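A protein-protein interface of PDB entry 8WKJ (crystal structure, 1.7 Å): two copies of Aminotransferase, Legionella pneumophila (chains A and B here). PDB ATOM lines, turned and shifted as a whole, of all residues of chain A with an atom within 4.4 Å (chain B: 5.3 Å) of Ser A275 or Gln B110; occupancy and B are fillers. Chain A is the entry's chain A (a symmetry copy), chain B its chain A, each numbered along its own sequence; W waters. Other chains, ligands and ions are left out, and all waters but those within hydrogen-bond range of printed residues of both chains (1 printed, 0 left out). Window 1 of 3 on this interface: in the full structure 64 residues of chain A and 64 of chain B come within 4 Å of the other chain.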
ATOM      1  N   GLN A 110      13.694   6.502  -2.642  1.00  0.00           N
ATOM      2  CA  GLN A 110      12.817   7.137  -1.659  1.00  0.00           C
ATOM      3  C   GLN A 110      11.678   6.218  -1.236  1.00  0.00           C
ATOM      4  O   GLN A 110      11.251   6.270  -0.081  1.00  0.00           O
ATOM      5  CB  GLN A 110      12.254   8.466  -2.178  1.00  0.00           C
ATOM      6  CG  GLN A 110      11.841   9.362  -0.992  1.00  0.00           C
ATOM      7  CD  GLN A 110      10.815  10.437  -1.314  1.00  0.00           C
ATOM      8  OE1 GLN A 110      10.091  10.362  -2.295  1.00  0.00           O
ATOM      9  NE2 GLN A 110      10.758  11.461  -0.463  1.00  0.00           N
ATOM     10  N   ILE A 271       5.511  10.494   5.701  1.00  0.00           N
ATOM     11  CA  ILE A 271       6.940  10.816   5.680  1.00  0.00           C
ATOM     12  C   ILE A 271       7.263  11.684   4.468  1.00  0.00           C
ATOM     13  O   ILE A 271       7.948  12.708   4.569  1.00  0.00           O
ATOM     14  CB  ILE A 271       7.795   9.537   5.675  1.00  0.00           C
ATOM     15  CG1 ILE A 271       7.488   8.662   6.896  1.00  0.00           C
ATOM     16  CG2 ILE A 271       9.274   9.916   5.642  1.00  0.00           C
ATOM     17  CD1 ILE A 271       7.914   9.302   8.229  1.00  0.00           C
ATOM     18  N   GLN A 272       6.757  11.286   3.304  1.00  0.00           N
ATOM     19  CA  GLN A 272       7.057  12.020   2.079  1.00  0.00           C
ATOM     20  C   GLN A 272       6.519  13.442   2.140  1.00  0.00           C
ATOM     21  O   GLN A 272       7.150  14.378   1.636  1.00  0.00           O
ATOM     22  CB  GLN A 272       6.472  11.263   0.889  1.00  0.00           C
ATOM     23  CG  GLN A 272       6.883  11.800  -0.469  1.00  0.00           C
ATOM     24  CD  GLN A 272       6.596  10.777  -1.538  1.00  0.00           C
ATOM     25  OE1 GLN A 272       6.980   9.620  -1.405  1.00  0.00           O
ATOM     26  NE2 GLN A 272       5.900  11.188  -2.585  1.00  0.00           N
ATOM     27  N   SER A 273       5.357  13.628   2.767  1.00  0.00           N
ATOM     28  CA  SER A 273       4.745  14.947   2.837  1.00  0.00           C
ATOM     29  C   SER A 273       5.532  15.889   3.738  1.00  0.00           C
ATOM     30  O   SER A 273       5.355  17.104   3.650  1.00  0.00           O
ATOM     31  CB  SER A 273       3.299  14.822   3.328  1.00  0.00           C
ATOM     32  OG  SER A 273       3.250  14.767   4.746  1.00  0.00           O
ATOM     33  N   GLN A 274       6.413  15.355   4.585  1.00  0.00           N
ATOM     34  CA  GLN A 274       7.246  16.177   5.453  1.00  0.00           C
ATOM     35  C   GLN A 274       8.702  16.171   5.026  1.00  0.00           C
ATOM     36  O   GLN A 274       9.558  16.677   5.763  1.00  0.00           O
ATOM     37  CB  GLN A 274       7.117  15.707   6.904  1.00  0.00           C
ATOM     38  CG  GLN A 274       5.686  15.774   7.453  1.00  0.00           C
ATOM     39  CD  GLN A 274       5.055  17.143   7.302  1.00  0.00           C
ATOM     40  OE1 GLN A 274       5.722  18.172   7.412  1.00  0.00           O
ATOM     41  NE2 GLN A 274       3.755  17.163   7.040  1.00  0.00           N
ATOM     42  N   SER A 275       9.007  15.641   3.842  1.00  0.00           N
ATOM     43  CA  SER A 275      10.398  15.586   3.410  1.00  0.00           C
ATOM     44  C   SER A 275      10.585  16.138   1.998  1.00  0.00           C
ATOM     45  O   SER A 275      11.460  16.969   1.782  1.00  0.00           O
ATOM     46  CB  SER A 275      10.929  14.154   3.503  1.00  0.00           C
ATOM     47  OG  SER A 275      10.085  13.220   2.826  1.00  0.00           O
ATOM     48  N   THR A 276       9.787  15.704   1.026  1.00  0.00           N
ATOM     49  CA  THR A 276       9.966  16.181  -0.341  1.00  0.00           C
ATOM     50  C   THR A 276       8.723  16.788  -0.959  1.00  0.00           C
ATOM     51  O   THR A 276       8.847  17.439  -2.004  1.00  0.00           O
ATOM     52  CB  THR A 276      10.410  15.048  -1.278  1.00  0.00           C
ATOM     53  OG1 THR A 276       9.444  13.987  -1.239  1.00  0.00           O
ATOM     54  CG2 THR A 276      11.808  14.535  -0.920  1.00  0.00           C
ATOM     55  N   SER A 277       7.549  16.586  -0.365  1.00  0.00           N
ATOM     56  CA  SER A 277       6.273  16.829  -1.057  1.00  0.00           C
ATOM     57  C   SER A 277       6.260  15.919  -2.288  1.00  0.00           C
ATOM     58  O   SER A 277       6.901  14.860  -2.297  1.00  0.00           O
ATOM     59  CB  SER A 277       6.071  18.319  -1.364  1.00  0.00           C
ATOM     60  OG  SER A 277       6.279  19.114  -0.207  1.00  0.00           O
ATOM     61  N   SER B 105      18.787  20.260  -2.970  1.00  0.00           N
ATOM     62  CA  SER B 105      17.885  19.227  -2.467  1.00  0.00           C
ATOM     63  C   SER B 105      16.559  19.247  -3.227  1.00  0.00           C
ATOM     64  O   SER B 105      16.295  20.135  -4.046  1.00  0.00           O
ATOM     65  CB  SER B 105      17.626  19.409  -0.959  1.00  0.00           C
ATOM     66  OG  SER B 105      18.833  19.257  -0.202  1.00  0.00           O
ATOM     67  N   VAL B 106      15.712  18.255  -2.925  1.00  0.00           N
ATOM     68  CA  VAL B 106      14.406  18.076  -3.574  1.00  0.00           C
ATOM     69  C   VAL B 106      13.402  19.011  -2.914  1.00  0.00           C
ATOM     70  O   VAL B 106      12.612  18.595  -2.053  1.00  0.00           O
ATOM     71  CB  VAL B 106      13.949  16.607  -3.492  1.00  0.00           C
ATOM     72  CG1 VAL B 106      12.594  16.397  -4.176  1.00  0.00           C
ATOM     73  CG2 VAL B 106      15.010  15.690  -4.115  1.00  0.00           C
ATOM     74  N   GLY B 107      13.426  20.275  -3.313  1.00  0.00           N
ATOM     75  CA  GLY B 107      12.655  21.294  -2.640  1.00  0.00           C
ATOM     76  C   GLY B 107      13.342  21.793  -1.379  1.00  0.00           C
ATOM     77  O   GLY B 107      14.198  21.131  -0.792  1.00  0.00           O
ATOM     78  N   GLY B 108      12.965  23.010  -0.970  1.00  0.00           N
ATOM     79  CA  GLY B 108      13.405  23.505   0.323  1.00  0.00           C
ATOM     80  C   GLY B 108      12.876  22.679   1.483  1.00  0.00           C
ATOM     81  O   GLY B 108      13.505  22.616   2.548  1.00  0.00           O
ATOM     82  N   LYS B 109      11.725  22.025   1.302  1.00  0.00           N
ATOM     83  CA  LYS B 109      11.256  21.106   2.339  1.00  0.00           C
ATOM     84  C   LYS B 109      12.299  20.038   2.625  1.00  0.00           C
ATOM     85  O   LYS B 109      12.547  19.701   3.789  1.00  0.00           O
ATOM     86  CB  LYS B 109       9.934  20.449   1.933  1.00  0.00           C
ATOM     87  CG  LYS B 109       9.345  19.562   3.052  1.00  0.00           C
ATOM     88  CD  LYS B 109       7.965  19.029   2.693  1.00  0.00           C
ATOM     89  CE  LYS B 109       6.876  20.080   2.890  1.00  0.00           C
ATOM     90  NZ  LYS B 109       5.535  19.586   2.408  1.00  0.00           N
ATOM     91  N   GLN B 110      12.943  19.503   1.576  1.00  0.00           N
ATOM     92  CA  GLN B 110      13.956  18.477   1.823  1.00  0.00           C
ATOM     93  C   GLN B 110      15.211  19.059   2.460  1.00  0.00           C
ATOM     94  O   GLN B 110      15.853  18.384   3.266  1.00  0.00           O
ATOM     95  CB  GLN B 110      14.320  17.722   0.539  1.00  0.00           C
ATOM     96  CG  GLN B 110      14.902  16.337   0.889  1.00  0.00           C
ATOM     97  CD  GLN B 110      15.774  15.706  -0.184  1.00  0.00           C
ATOM     98  OE1 GLN B 110      16.293  16.373  -1.065  1.00  0.00           O
ATOM     99  NE2 GLN B 110      15.934  14.385  -0.102  1.00  0.00           N
ATOM    100  N   SER B 111      15.583  20.298   2.122  1.00  0.00           N
ATOM    101  CA  SER B 111      16.664  20.934   2.866  1.00  0.00           C
ATOM    102  C   SER B 111      16.364  20.902   4.361  1.00  0.00           C
ATOM    103  O   SER B 111      17.212  20.519   5.178  1.00  0.00           O
ATOM    104  CB  SER B 111      16.856  22.382   2.410  1.00  0.00           C
ATOM    105  OG  SER B 111      17.151  22.454   1.032  1.00  0.00           O
ATOM    106  N   CYS B 112      15.143  21.300   4.730  1.00  0.00           N
ATOM    107  CA  CYS B 112      14.774  21.355   6.145  1.00  0.00           C
ATOM    108  C   CYS B 112      14.735  19.963   6.761  1.00  0.00           C
ATOM    109  O   CYS B 112      15.209  19.754   7.888  1.00  0.00           O
ATOM    110  CB  CYS B 112      13.410  22.022   6.306  1.00  0.00           C
ATOM    111  SG  CYS B 112      13.328  23.763   5.861  1.00  0.00           S
ATOM    112  N   TYR B 113      14.156  19.002   6.040  1.00  0.00           N
ATOM    113  CA  TYR B 113      14.043  17.645   6.564  1.00  0.00           C
ATOM    114  C   TYR B 113      15.420  17.005   6.709  1.00  0.00           C
ATOM    115  O   TYR B 113      15.727  16.389   7.741  1.00  0.00           O
ATOM    116  CB  TYR B 113      13.128  16.813   5.649  1.00  0.00           C
ATOM    117  CG  TYR B 113      13.083  15.351   6.034  1.00  0.00           C
ATOM    118  CD1 TYR B 113      12.156  14.889   6.958  1.00  0.00           C
ATOM    119  CD2 TYR B 113      13.993  14.444   5.503  1.00  0.00           C
ATOM    120  CE1 TYR B 113      12.126  13.556   7.341  1.00  0.00           C
ATOM    121  CE2 TYR B 113      13.967  13.102   5.873  1.00  0.00           C
ATOM    122  CZ  TYR B 113      13.037  12.666   6.795  1.00  0.00           C
ATOM    123  OH  TYR B 113      13.017  11.337   7.181  1.00  0.00           O
ATOM    124  N   ASN B 114      16.273  17.149   5.685  1.00  0.00           N
ATOM    125  CA  ASN B 114      17.646  16.644   5.770  1.00  0.00           C
ATOM    126  C   ASN B 114      18.387  17.252   6.955  1.00  0.00           C
ATOM    127  O   ASN B 114      19.143  16.562   7.647  1.00  0.00           O
ATOM    128  CB  ASN B 114      18.415  16.962   4.484  1.00  0.00           C
ATOM    129  CG  ASN B 114      17.997  16.094   3.305  1.00  0.00           C
ATOM    130  OD1 ASN B 114      17.378  15.048   3.475  1.00  0.00           O
ATOM    131  ND2 ASN B 114      18.323  16.550   2.098  1.00  0.00           N
ATOM    132  N   LEU B 115      18.211  18.554   7.173  1.00  0.00           N
ATOM    133  CA  LEU B 115      18.815  19.217   8.322  1.00  0.00           C
ATOM    134  C   LEU B 115      18.405  18.547   9.630  1.00  0.00           C
ATOM    135  O   LEU B 115      19.252  18.222  10.478  1.00  0.00           O
ATOM    136  CB  LEU B 115      18.409  20.693   8.316  1.00  0.00           C
ATOM    137  CG  LEU B 115      18.716  21.454   9.603  1.00  0.00           C
ATOM    138  CD1 LEU B 115      20.229  21.464   9.870  1.00  0.00           C
ATOM    139  CD2 LEU B 115      18.157  22.872   9.486  1.00  0.00           C
ATOM    140  N   GLN B 272      20.604  12.627   2.207  1.00  0.00           N
ATOM    141  CA  GLN B 272      20.021  12.708   0.871  1.00  0.00           C
ATOM    142  C   GLN B 272      20.471  11.544   0.001  1.00  0.00           C
ATOM    143  O   GLN B 272      19.695  11.026  -0.811  1.00  0.00           O
ATOM    144  CB  GLN B 272      20.406  14.044   0.240  1.00  0.00           C
ATOM    145  CG  GLN B 272      19.702  14.355  -1.067  1.00  0.00           C
ATOM    146  CD  GLN B 272      19.835  15.821  -1.391  1.00  0.00           C
ATOM    147  OE1 GLN B 272      19.559  16.668  -0.548  1.00  0.00           O
ATOM    148  NE2 GLN B 272      20.284  16.127  -2.596  1.00  0.00           N
ATOM    149  N   SER B 275      18.235   8.615   0.592  1.00  0.00           N
ATOM    150  CA  SER B 275      16.792   8.820   0.554  1.00  0.00           C
ATOM    151  C   SER B 275      16.295   9.163  -0.849  1.00  0.00           C
ATOM    152  O   SER B 275      15.344   8.551  -1.323  1.00  0.00           O
ATOM    153  CB  SER B 275      16.381   9.905   1.551  1.00  0.00           C
ATOM    154  OG  SER B 275      17.132  11.108   1.379  1.00  0.00           O
ATOM    155  N   THR B 276      16.911  10.123  -1.533  1.00  0.00           N
ATOM    156  CA  THR B 276      16.436  10.504  -2.859  1.00  0.00           C
ATOM    157  C   THR B 276      17.491  10.438  -3.944  1.00  0.00           C
ATOM    158  O   THR B 276      17.123  10.495  -5.124  1.00  0.00           O
ATOM    159  CB  THR B 276      15.888  11.937  -2.870  1.00  0.00           C
ATOM    160  OG1 THR B 276      16.907  12.845  -2.424  1.00  0.00           O
ATOM    161  CG2 THR B 276      14.623  12.064  -2.015  1.00  0.00           C
HETATM  162  O   HOH W   1      13.536  12.374   1.445  1.00  0.00           O
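The side-chain hydroxyl of Ser A277 lies within hydrogen-bond range of the side-chain amino group of Lys B109 (2.8 Å). The backbone carbonyl oxygen of Ser B275 lies close to the backbone NH of Gln A110. NZ of Lys B109 is in hydrogen-bond range of O of Ser A273 (2.8 Å). The backbone NH (N) of Gln B110 lies close to the backbone carbonyl oxygen (O) of Ser A275, at 2.9 Å.
OG1 of Thr B276 sits at hydrogen-bond distance from NE2 of Gln B110 (3.0 Å). OE1 of Gln A110 lies close to OE1 of Gln A272, at 3.3 Å. The side-chain amide oxygen (OE1) of Gln B110 lies close to the side-chain amide oxygen (OE1) of Gln B272. The side-chain hydroxyl (OG) of Ser A273 is in hydrogen-bond range of the side-chain amide nitrogen (NE2) of Gln A274 (3.4 Å). O of Gln B272 sits close to OG of Ser B275 (3.4 Å). O of Gln A272 sits close to OG of Ser A275 (3.4 Å).
Gln A274 touches Lys B109 (C to CD, 3.8 Å). Tyr B113 touches Gln A274. Ser A275 touches Lys B109. CB of Ser A275 touches CG of Tyr B113, 3.5 Å away. Val B106 touches Thr A276 (CG1 to CG2, 3.8 Å). Thr A276 touches Thr B276.
Printed residues of chain B within 4 Å of Ser A275: Lys B109 (3.3 Å), Gln B110 (2.9 Å) and Tyr B113 (3.5 Å). Of the printed residues of chain A, Gln B110 touches Ser A275. Of the printed residues of chain B, Ser A273 touches Lys B109. Of the printed residues of chain A, Thr B276 touches Thr A276 (3.9 Å).
Of the 14 printed residues of chain B, 6 touch a printed residue of chain A. Printed residues of chain B that touch a printed residue of chain A: Val B106, Lys B109, Gln B110, Tyr B113, Ser B275 and Thr B276. Hydrophobic or aromatic side chains of chain B within 4 Å of the printed part of chain A: Val B106 and Tyr B113. Of the 8 printed residues of chain A, 6 touch a printed residue of chain B. Printed residues of chain A that touch a printed residue of chain B: Gln A110, Ser A273, Gln A274, Ser A275, Thr A276 and Ser A277. Among the printed residues, no Asp or Glu carboxylate lies within 4 Å of a Lys or Arg side-chain nitrogen of the other chain.
Gln A110 touches Ser B275, and with the chains exchanged Ser A275 touches Gln B110. Thr A276 touches its own counterpart, Thr B276. Of the 10 pairs that touch across the chains among the printed residues, 3 have their exchanged pair printed and touching as well.
Water W1 lies within hydrogen-bond range of NE2 of Gln A110 and NE2 of Gln B110.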
